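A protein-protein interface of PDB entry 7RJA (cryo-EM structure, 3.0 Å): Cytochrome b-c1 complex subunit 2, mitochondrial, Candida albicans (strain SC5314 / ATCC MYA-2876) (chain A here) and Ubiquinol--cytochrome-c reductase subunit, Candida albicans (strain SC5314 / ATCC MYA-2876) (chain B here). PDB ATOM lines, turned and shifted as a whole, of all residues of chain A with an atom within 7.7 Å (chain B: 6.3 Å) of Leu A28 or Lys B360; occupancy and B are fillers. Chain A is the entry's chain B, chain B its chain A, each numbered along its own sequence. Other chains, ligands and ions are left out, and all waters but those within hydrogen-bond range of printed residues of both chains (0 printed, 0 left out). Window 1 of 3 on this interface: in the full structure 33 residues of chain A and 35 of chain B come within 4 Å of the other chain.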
ATOM      1  N   LYS A  22      29.532   8.546  -8.191  1.00  0.00           N
ATOM      2  CA  LYS A  22      29.154   9.677  -7.358  1.00  0.00           C
ATOM      3  C   LYS A  22      29.456   9.348  -5.905  1.00  0.00           C
ATOM      4  O   LYS A  22      29.419   8.182  -5.507  1.00  0.00           O
ATOM      5  CB  LYS A  22      27.674  10.020  -7.543  1.00  0.00           C
ATOM      6  CG  LYS A  22      26.738   8.880  -7.211  1.00  0.00           C
ATOM      7  CD  LYS A  22      25.307   9.219  -7.577  1.00  0.00           C
ATOM      8  CE  LYS A  22      24.372   8.070  -7.257  1.00  0.00           C
ATOM      9  NZ  LYS A  22      24.653   6.878  -8.106  1.00  0.00           N
ATOM     10  N   GLU A  23      29.751  10.381  -5.121  1.00  0.00           N
ATOM     11  CA  GLU A  23      30.181  10.178  -3.746  1.00  0.00           C
ATOM     12  C   GLU A  23      29.070   9.546  -2.920  1.00  0.00           C
ATOM     13  O   GLU A  23      27.882   9.682  -3.224  1.00  0.00           O
ATOM     14  CB  GLU A  23      30.612  11.508  -3.123  1.00  0.00           C
ATOM     15  CG  GLU A  23      31.741  12.200  -3.870  1.00  0.00           C
ATOM     16  CD  GLU A  23      32.909  11.274  -4.152  1.00  0.00           C
ATOM     17  OE1 GLU A  23      33.208  10.416  -3.297  1.00  0.00           O
ATOM     18  OE2 GLU A  23      33.524  11.401  -5.231  1.00  0.00           O
ATOM     19  N   SER A  24      29.472   8.849  -1.861  1.00  0.00           N
ATOM     20  CA  SER A  24      28.568   8.103  -1.003  1.00  0.00           C
ATOM     21  C   SER A  24      28.732   8.552   0.443  1.00  0.00           C
ATOM     22  O   SER A  24      29.786   9.047   0.849  1.00  0.00           O
ATOM     23  CB  SER A  24      28.825   6.597  -1.104  1.00  0.00           C
ATOM     24  OG  SER A  24      29.881   6.210  -0.243  1.00  0.00           O
ATOM     25  N   ALA A  25      27.666   8.360   1.220  1.00  0.00           N
ATOM     26  CA  ALA A  25      27.661   8.816   2.605  1.00  0.00           C
ATOM     27  C   ALA A  25      28.513   7.927   3.507  1.00  0.00           C
ATOM     28  O   ALA A  25      29.230   8.432   4.377  1.00  0.00           O
ATOM     29  CB  ALA A  25      26.226   8.873   3.125  1.00  0.00           C
ATOM     30  N   THR A  26      28.452   6.609   3.314  1.00  0.00           N
ATOM     31  CA  THR A  26      29.006   5.645   4.258  1.00  0.00           C
ATOM     32  C   THR A  26      30.311   5.020   3.775  1.00  0.00           C
ATOM     33  O   THR A  26      30.534   3.826   3.991  1.00  0.00           O
ATOM     34  CB  THR A  26      27.981   4.548   4.545  1.00  0.00           C
ATOM     35  OG1 THR A  26      28.457   3.714   5.608  1.00  0.00           O
ATOM     36  CG2 THR A  26      27.730   3.700   3.301  1.00  0.00           C
ATOM     37  N   ASP A  27      31.141   5.789   3.068  1.00  0.00           N
ATOM     38  CA  ASP A  27      32.496   5.413   2.657  1.00  0.00           C
ATOM     39  C   ASP A  27      32.591   3.938   2.279  1.00  0.00           C
ATOM     40  O   ASP A  27      33.584   3.275   2.591  1.00  0.00           O
ATOM     41  CB  ASP A  27      33.548   5.765   3.727  1.00  0.00           C
ATOM     42  CG  ASP A  27      33.373   5.018   5.038  1.00  0.00           C
ATOM     43  OD1 ASP A  27      32.430   4.232   5.200  1.00  0.00           O
ATOM     44  OD2 ASP A  27      34.216   5.230   5.933  1.00  0.00           O
ATOM     45  N   LEU A  28      31.556   3.418   1.625  1.00  0.00           N
ATOM     46  CA  LEU A  28      31.595   2.124   0.961  1.00  0.00           C
ATOM     47  C   LEU A  28      31.407   2.349  -0.526  1.00  0.00           C
ATOM     48  O   LEU A  28      30.501   3.080  -0.937  1.00  0.00           O
ATOM     49  CB  LEU A  28      30.506   1.176   1.468  1.00  0.00           C
ATOM     50  CG  LEU A  28      30.655   0.562   2.851  1.00  0.00           C
ATOM     51  CD1 LEU A  28      29.500  -0.386   3.098  1.00  0.00           C
ATOM     52  CD2 LEU A  28      31.975  -0.159   2.991  1.00  0.00           C
ATOM     53  N   THR A  29      32.254   1.724  -1.330  1.00  0.00           N
ATOM     54  CA  THR A  29      32.130   1.827  -2.778  1.00  0.00           C
ATOM     55  C   THR A  29      31.120   0.782  -3.229  1.00  0.00           C
ATOM     56  O   THR A  29      31.476  -0.324  -3.633  1.00  0.00           O
ATOM     57  CB  THR A  29      33.479   1.631  -3.450  1.00  0.00           C
ATOM     58  OG1 THR A  29      34.340   2.726  -3.123  1.00  0.00           O
ATOM     59  CG2 THR A  29      33.310   1.565  -4.949  1.00  0.00           C
ATOM     60  N   LYS A  30      29.838   1.136  -3.165  1.00  0.00           N
ATOM     61  CA  LYS A  30      28.766   0.214  -3.536  1.00  0.00           C
ATOM     62  C   LYS A  30      28.722   0.110  -5.057  1.00  0.00           C
ATOM     63  O   LYS A  30      27.781   0.545  -5.722  1.00  0.00           O
ATOM     64  CB  LYS A  30      27.432   0.677  -2.968  1.00  0.00           C
ATOM     65  CG  LYS A  30      27.360   0.638  -1.455  1.00  0.00           C
ATOM     66  CD  LYS A  30      25.970   0.983  -0.945  1.00  0.00           C
ATOM     67  CE  LYS A  30      25.660   2.461  -1.102  1.00  0.00           C
ATOM     68  NZ  LYS A  30      26.523   3.315  -0.240  1.00  0.00           N
ATOM     69  N   LEU A  31      29.770  -0.489  -5.612  1.00  0.00           N
ATOM     70  CA  LEU A  31      29.841  -0.699  -7.047  1.00  0.00           C
ATOM     71  C   LEU A  31      28.754  -1.668  -7.498  1.00  0.00           C
ATOM     72  O   LEU A  31      28.370  -2.593  -6.779  1.00  0.00           O
ATOM     73  CB  LEU A  31      31.217  -1.236  -7.437  1.00  0.00           C
ATOM     74  CG  LEU A  31      31.456  -1.496  -8.922  1.00  0.00           C
ATOM     75  CD1 LEU A  31      31.341  -0.223  -9.724  1.00  0.00           C
ATOM     76  CD2 LEU A  31      32.816  -2.115  -9.121  1.00  0.00           C
ATOM     77  N   GLY A  75      36.625  -8.216   2.828  1.00  0.00           N
ATOM     78  CA  GLY A  75      35.471  -7.698   3.526  1.00  0.00           C
ATOM     79  C   GLY A  75      34.296  -7.348   2.646  1.00  0.00           C
ATOM     80  O   GLY A  75      33.236  -6.992   3.174  1.00  0.00           O
ATOM     81  N   GLY A  76      34.435  -7.449   1.336  1.00  0.00           N
ATOM     82  CA  GLY A  76      33.364  -7.051   0.458  1.00  0.00           C
ATOM     83  C   GLY A  76      32.264  -8.087   0.360  1.00  0.00           C
ATOM     84  O   GLY A  76      32.422  -9.254   0.713  1.00  0.00           O
ATOM     85  N   THR A  77      31.122  -7.623  -0.128  1.00  0.00           N
ATOM     86  CA  THR A  77      29.961  -8.448  -0.406  1.00  0.00           C
ATOM     87  C   THR A  77      29.654  -8.356  -1.890  1.00  0.00           C
ATOM     88  O   THR A  77      29.929  -7.338  -2.530  1.00  0.00           O
ATOM     89  CB  THR A  77      28.742  -7.992   0.405  1.00  0.00           C
ATOM     90  OG1 THR A  77      29.030  -8.082   1.805  1.00  0.00           O
ATOM     91  CG2 THR A  77      27.526  -8.846   0.086  1.00  0.00           C
ATOM     92  N   GLU A  79      26.563  -9.831  -4.866  1.00  0.00           N
ATOM     93  CA  GLU A  79      25.367 -10.590  -5.185  1.00  0.00           C
ATOM     94  C   GLU A  79      24.978 -10.311  -6.627  1.00  0.00           C
ATOM     95  O   GLU A  79      25.413  -9.330  -7.227  1.00  0.00           O
ATOM     96  CB  GLU A  79      24.203 -10.250  -4.245  1.00  0.00           C
ATOM     97  CG  GLU A  79      23.730  -8.810  -4.317  1.00  0.00           C
ATOM     98  CD  GLU A  79      22.304  -8.641  -3.828  1.00  0.00           C
ATOM     99  OE1 GLU A  79      21.705  -9.638  -3.373  1.00  0.00           O
ATOM    100  OE2 GLU A  79      21.777  -7.511  -3.908  1.00  0.00           O
ATOM    101  N   THR A  91      28.087  -5.093  -5.843  1.00  0.00           N
ATOM    102  CA  THR A  91      29.231  -5.314  -4.976  1.00  0.00           C
ATOM    103  C   THR A  91      29.307  -4.170  -3.980  1.00  0.00           C
ATOM    104  O   THR A  91      28.841  -3.062  -4.247  1.00  0.00           O
ATOM    105  CB  THR A  91      30.537  -5.409  -5.763  1.00  0.00           C
ATOM    106  OG1 THR A  91      30.586  -4.360  -6.733  1.00  0.00           O
ATOM    107  CG2 THR A  91      30.636  -6.746  -6.464  1.00  0.00           C
ATOM    108  N   THR A  92      29.892  -4.456  -2.822  1.00  0.00           N
ATOM    109  CA  THR A  92      29.978  -3.480  -1.742  1.00  0.00           C
ATOM    110  C   THR A  92      31.275  -3.722  -0.994  1.00  0.00           C
ATOM    111  O   THR A  92      31.481  -4.812  -0.459  1.00  0.00           O
ATOM    112  CB  THR A  92      28.781  -3.605  -0.802  1.00  0.00           C
ATOM    113  OG1 THR A  92      27.592  -3.184  -1.478  1.00  0.00           O
ATOM    114  CG2 THR A  92      28.981  -2.756   0.435  1.00  0.00           C
ATOM    115  N   PHE A  93      32.140  -2.717  -0.941  1.00  0.00           N
ATOM    116  CA  PHE A  93      33.456  -2.918  -0.355  1.00  0.00           C
ATOM    117  C   PHE A  93      34.006  -1.585   0.119  1.00  0.00           C
ATOM    118  O   PHE A  93      33.494  -0.520  -0.227  1.00  0.00           O
ATOM    119  CB  PHE A  93      34.410  -3.559  -1.360  1.00  0.00           C
ATOM    120  CG  PHE A  93      34.301  -2.983  -2.734  1.00  0.00           C
ATOM    121  CD1 PHE A  93      35.037  -1.874  -3.092  1.00  0.00           C
ATOM    122  CD2 PHE A  93      33.452  -3.541  -3.664  1.00  0.00           C
ATOM    123  CE1 PHE A  93      34.936  -1.342  -4.352  1.00  0.00           C
ATOM    124  CE2 PHE A  93      33.349  -3.011  -4.926  1.00  0.00           C
ATOM    125  CZ  PHE A  93      34.090  -1.911  -5.269  1.00  0.00           C
ATOM    126  N   LEU A  94      35.061  -1.667   0.922  1.00  0.00           N
ATOM    127  CA  LEU A  94      35.723  -0.471   1.409  1.00  0.00           C
ATOM    128  C   LEU A  94      36.383   0.267   0.249  1.00  0.00           C
ATOM    129  O   LEU A  94      36.710  -0.315  -0.787  1.00  0.00           O
ATOM    130  CB  LEU A  94      36.755  -0.843   2.470  1.00  0.00           C
ATOM    131  CG  LEU A  94      36.166  -1.439   3.750  1.00  0.00           C
ATOM    132  CD1 LEU A  94      37.268  -1.954   4.647  1.00  0.00           C
ATOM    133  CD2 LEU A  94      35.324  -0.420   4.488  1.00  0.00           C
ATOM    134  N   LYS A  95      36.581   1.572   0.433  1.00  0.00           N
ATOM    135  CA  LYS A  95      37.074   2.401  -0.659  1.00  0.00           C
ATOM    136  C   LYS A  95      38.429   1.941  -1.172  1.00  0.00           C
ATOM    137  O   LYS A  95      38.773   2.233  -2.321  1.00  0.00           O
ATOM    138  CB  LYS A  95      37.169   3.858  -0.208  1.00  0.00           C
ATOM    139  CG  LYS A  95      35.825   4.517   0.042  1.00  0.00           C
ATOM    140  CD  LYS A  95      35.979   5.942   0.560  1.00  0.00           C
ATOM    141  CE  LYS A  95      36.494   6.895  -0.510  1.00  0.00           C
ATOM    142  NZ  LYS A  95      35.498   7.109  -1.594  1.00  0.00           N
ATOM    143  N   ALA A 189      28.472   3.189  -9.679  1.00  0.00           N
ATOM    144  CA  ALA A 189      29.186   3.100  -8.418  1.00  0.00           C
ATOM    145  C   ALA A 189      28.771   4.260  -7.529  1.00  0.00           C
ATOM    146  O   ALA A 189      28.377   5.324  -8.007  1.00  0.00           O
ATOM    147  CB  ALA A 189      30.704   3.116  -8.626  1.00  0.00           C
ATOM    148  N   GLU A 190      28.867   4.040  -6.222  1.00  0.00           N
ATOM    149  CA  GLU A 190      28.573   5.064  -5.230  1.00  0.00           C
ATOM    150  C   GLU A 190      29.748   5.157  -4.276  1.00  0.00           C
ATOM    151  O   GLU A 190      29.997   4.225  -3.505  1.00  0.00           O
ATOM    152  CB  GLU A 190      27.288   4.745  -4.466  1.00  0.00           C
ATOM    153  CG  GLU A 190      26.034   5.307  -5.105  1.00  0.00           C
ATOM    154  CD  GLU A 190      24.846   5.288  -4.165  1.00  0.00           C
ATOM    155  OE1 GLU A 190      24.984   4.765  -3.040  1.00  0.00           O
ATOM    156  OE2 GLU A 190      23.773   5.799  -4.549  1.00  0.00           O
ATOM    157  N   GLY A 191      30.461   6.275  -4.318  1.00  0.00           N
ATOM    158  CA  GLY A 191      31.594   6.477  -3.440  1.00  0.00           C
ATOM    159  C   GLY A 191      32.903   6.054  -4.066  1.00  0.00           C
ATOM    160  O   GLY A 191      33.797   5.556  -3.379  1.00  0.00           O
ATOM    161  N   ALA A 192      33.028   6.253  -5.374  1.00  0.00           N
ATOM    162  CA  ALA A 192      34.262   5.958  -6.084  1.00  0.00           C
ATOM    163  C   ALA A 192      34.512   7.069  -7.089  1.00  0.00           C
ATOM    164  O   ALA A 192      33.593   7.488  -7.793  1.00  0.00           O
ATOM    165  CB  ALA A 192      34.191   4.606  -6.795  1.00  0.00           C
ATOM    166  N   LYS B 355      33.975  -4.318   9.670  1.00  0.00           N
ATOM    167  CA  LYS B 355      34.013  -2.945   9.185  1.00  0.00           C
ATOM    168  C   LYS B 355      32.973  -2.728   8.094  1.00  0.00           C
ATOM    169  O   LYS B 355      32.239  -1.729   8.108  1.00  0.00           O
ATOM    170  CB  LYS B 355      35.411  -2.612   8.674  1.00  0.00           C
ATOM    171  CG  LYS B 355      36.456  -2.561   9.768  1.00  0.00           C
ATOM    172  CD  LYS B 355      37.858  -2.703   9.216  1.00  0.00           C
ATOM    173  CE  LYS B 355      38.211  -1.558   8.296  1.00  0.00           C
ATOM    174  NZ  LYS B 355      39.600  -1.675   7.787  1.00  0.00           N
ATOM    175  N   THR B 356      32.876  -3.665   7.151  1.00  0.00           N
ATOM    176  CA  THR B 356      31.895  -3.530   6.082  1.00  0.00           C
ATOM    177  C   THR B 356      30.472  -3.583   6.620  1.00  0.00           C
ATOM    178  O   THR B 356      29.603  -2.839   6.156  1.00  0.00           O
ATOM    179  CB  THR B 356      32.109  -4.615   5.032  1.00  0.00           C
ATOM    180  OG1 THR B 356      33.402  -4.457   4.442  1.00  0.00           O
ATOM    181  CG2 THR B 356      31.051  -4.524   3.952  1.00  0.00           C
ATOM    182  N   ALA B 357      30.206  -4.459   7.588  1.00  0.00           N
ATOM    183  CA  ALA B 357      28.869  -4.538   8.165  1.00  0.00           C
ATOM    184  C   ALA B 357      28.513  -3.260   8.908  1.00  0.00           C
ATOM    185  O   ALA B 357      27.375  -2.787   8.827  1.00  0.00           O
ATOM    186  CB  ALA B 357      28.769  -5.744   9.094  1.00  0.00           C
ATOM    187  N   LEU B 358      29.465  -2.691   9.649  1.00  0.00           N
ATOM    188  CA  LEU B 358      29.209  -1.421  10.315  1.00  0.00           C
ATOM    189  C   LEU B 358      28.899  -0.332   9.304  1.00  0.00           C
ATOM    190  O   LEU B 358      27.984   0.472   9.508  1.00  0.00           O
ATOM    191  CB  LEU B 358      30.409  -1.016  11.169  1.00  0.00           C
ATOM    192  CG  LEU B 358      30.664  -1.836  12.430  1.00  0.00           C
ATOM    193  CD1 LEU B 358      31.969  -1.406  13.065  1.00  0.00           C
ATOM    194  CD2 LEU B 358      29.518  -1.684  13.412  1.00  0.00           C
ATOM    195  N   ALA B 359      29.651  -0.285   8.206  1.00  0.00           N
ATOM    196  CA  ALA B 359      29.398   0.753   7.216  1.00  0.00           C
ATOM    197  C   ALA B 359      28.070   0.536   6.503  1.00  0.00           C
ATOM    198  O   ALA B 359      27.398   1.506   6.144  1.00  0.00           O
ATOM    199  CB  ALA B 359      30.542   0.810   6.212  1.00  0.00           C
ATOM    200  N   LYS B 360      27.677  -0.720   6.285  1.00  0.00           N
ATOM    201  CA  LYS B 360      26.373  -0.996   5.691  1.00  0.00           C
ATOM    202  C   LYS B 360      25.246  -0.582   6.624  1.00  0.00           C
ATOM    203  O   LYS B 360      24.251   0.004   6.185  1.00  0.00           O
ATOM    204  CB  LYS B 360      26.249  -2.479   5.355  1.00  0.00           C
ATOM    205  CG  LYS B 360      26.853  -2.874   4.021  1.00  0.00           C
ATOM    206  CD  LYS B 360      26.434  -4.279   3.610  1.00  0.00           C
ATOM    207  CE  LYS B 360      24.967  -4.343   3.199  1.00  0.00           C
ATOM    208  NZ  LYS B 360      24.509  -5.740   2.968  1.00  0.00           N
ATOM    209  N   GLU B 361      25.385  -0.881   7.914  1.00  0.00           N
ATOM    210  CA  GLU B 361      24.351  -0.546   8.882  1.00  0.00           C
ATOM    211  C   GLU B 361      24.137   0.953   9.008  1.00  0.00           C
ATOM    212  O   GLU B 361      23.103   1.377   9.531  1.00  0.00           O
ATOM    213  CB  GLU B 361      24.726  -1.126  10.244  1.00  0.00           C
ATOM    214  CG  GLU B 361      23.621  -1.101  11.270  1.00  0.00           C
ATOM    215  CD  GLU B 361      24.029  -1.786  12.558  1.00  0.00           C
ATOM    216  OE1 GLU B 361      24.425  -2.969  12.503  1.00  0.00           O
ATOM    217  OE2 GLU B 361      23.957  -1.142  13.626  1.00  0.00           O
ATOM    218  N   LEU B 362      25.088   1.765   8.544  1.00  0.00           N
ATOM    219  CA  LEU B 362      25.049   3.209   8.729  1.00  0.00           C
ATOM    220  C   LEU B 362      24.870   3.955   7.414  1.00  0.00           C
ATOM    221  O   LEU B 362      25.326   5.095   7.287  1.00  0.00           O
ATOM    222  CB  LEU B 362      26.325   3.677   9.427  1.00  0.00           C
ATOM    223  CG  LEU B 362      26.515   3.185  10.861  1.00  0.00           C
ATOM    224  CD1 LEU B 362      27.877   3.606  11.379  1.00  0.00           C
ATOM    225  CD2 LEU B 362      25.421   3.690  11.777  1.00  0.00           C
ATOM    226  N   ALA B 363      24.226   3.334   6.427  1.00  0.00           N
ATOM    227  CA  ALA B 363      24.003   3.981   5.139  1.00  0.00           C
ATOM    228  C   ALA B 363      22.672   4.726   5.117  1.00  0.00           C
ATOM    229  O   ALA B 363      22.635   5.942   4.907  1.00  0.00           O
ATOM    230  CB  ALA B 363      24.054   2.941   4.015  1.00  0.00           C
ATOM    231  N   ASN B 364      21.575   4.010   5.338  1.00  0.00           N
ATOM    232  CA  ASN B 364      20.264   4.637   5.325  1.00  0.00           C
ATOM    233  C   ASN B 364      20.172   5.682   6.429  1.00  0.00           C
ATOM    234  O   ASN B 364      20.608   5.454   7.560  1.00  0.00           O
ATOM    235  CB  ASN B 364      19.177   3.576   5.505  1.00  0.00           C
ATOM    236  CG  ASN B 364      17.891   3.923   4.776  1.00  0.00           C
ATOM    237  OD1 ASN B 364      17.898   4.664   3.794  1.00  0.00           O
ATOM    238  ND2 ASN B 364      16.779   3.378   5.253  1.00  0.00           N
ATOM    239  N   ALA B 367      18.600   4.437   9.527  1.00  0.00           N
ATOM    240  CA  ALA B 367      19.502   3.651  10.358  1.00  0.00           C
ATOM    241  C   ALA B 367      20.490   4.542  11.094  1.00  0.00           C
ATOM    242  O   ALA B 367      20.805   4.291  12.260  1.00  0.00           O
ATOM    243  CB  ALA B 367      20.241   2.625   9.505  1.00  0.00           C
ATOM    244  N   PHE B 389      36.529   2.194  12.705  1.00  0.00           N
ATOM    245  CA  PHE B 389      37.459   1.482  11.837  1.00  0.00           C
ATOM    246  C   PHE B 389      38.852   1.447  12.445  1.00  0.00           C
ATOM    247  O   PHE B 389      39.522   0.409  12.424  1.00  0.00           O
ATOM    248  CB  PHE B 389      37.503   2.141  10.460  1.00  0.00           C
ATOM    249  CG  PHE B 389      36.325   1.817   9.586  1.00  0.00           C
ATOM    250  CD1 PHE B 389      35.212   1.173  10.092  1.00  0.00           C
ATOM    251  CD2 PHE B 389      36.336   2.160   8.248  1.00  0.00           C
ATOM    252  CE1 PHE B 389      34.139   0.879   9.282  1.00  0.00           C
ATOM    253  CE2 PHE B 389      35.266   1.867   7.435  1.00  0.00           C
ATOM    254  CZ  PHE B 389      34.166   1.226   7.953  1.00  0.00           C
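O of Gly A75 is in hydrogen-bond range of OG1 of Thr B356 (2.8 Å). The backbone carbonyl oxygen of Ala B359 sits at hydrogen-bond distance from the side-chain hydroxyl of Thr A26, at 2.5 Å.
The side-chain hydroxyl (OG) of Ser A24 lies within hydrogen-bond range of the backbone carbonyl oxygen (O) of Leu A28, 3.3 Å away.
Thr A26 touches Leu B362 (OG1 to O, 3.8 Å). CB of Ala B363 touches CG2 of Thr A26, 3.8 Å away. Phe B389 touches Asp A27. Leu A28 touches Thr B356. Ala B359 touches Leu A28. Lys B360 touches Leu A28. CE of Lys B355 touches CD1 of Leu A94, 3.8 Å away. Phe B389 touches Leu A94.
Of chain B, only Thr B356 (3.9 Å), Ala B359 (3.4 Å) and Lys B360 (3.7 Å) come within 4 Å of Leu A28. Lys B360 touches one residue of chain A. Printed residues of chain A within 4 Å of Phe B389: Asp A27 (3.8 Å) and Leu A94 (3.7 Å). Printed residues of chain B within 4 Å of Asp A27: Phe B389. Thr A77 touches none of the printed residues of chain B. Thr A92 touches none of the printed residues of chain B. The nearest residue of chain B that does not touch Leu A28 is Lys B355 (5.4 Å). The nearest residue of chain A that does not touch Lys B360 is Thr A92 (4.2 Å). The nearest printed residue of chain B that does not touch Thr A26 is Lys B360 (4.6 Å).
Of the 23 printed residues of chain A, 5 touch a printed residue of chain B. Hydrophobic or aromatic side chains of chain A within 4 Å of the printed part of chain B: Leu A28 and Leu A94. Among the printed residues, no Asp or Glu carboxylate lies within 4 Å of a Lys or Arg side-chain nitrogen of the other chain.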
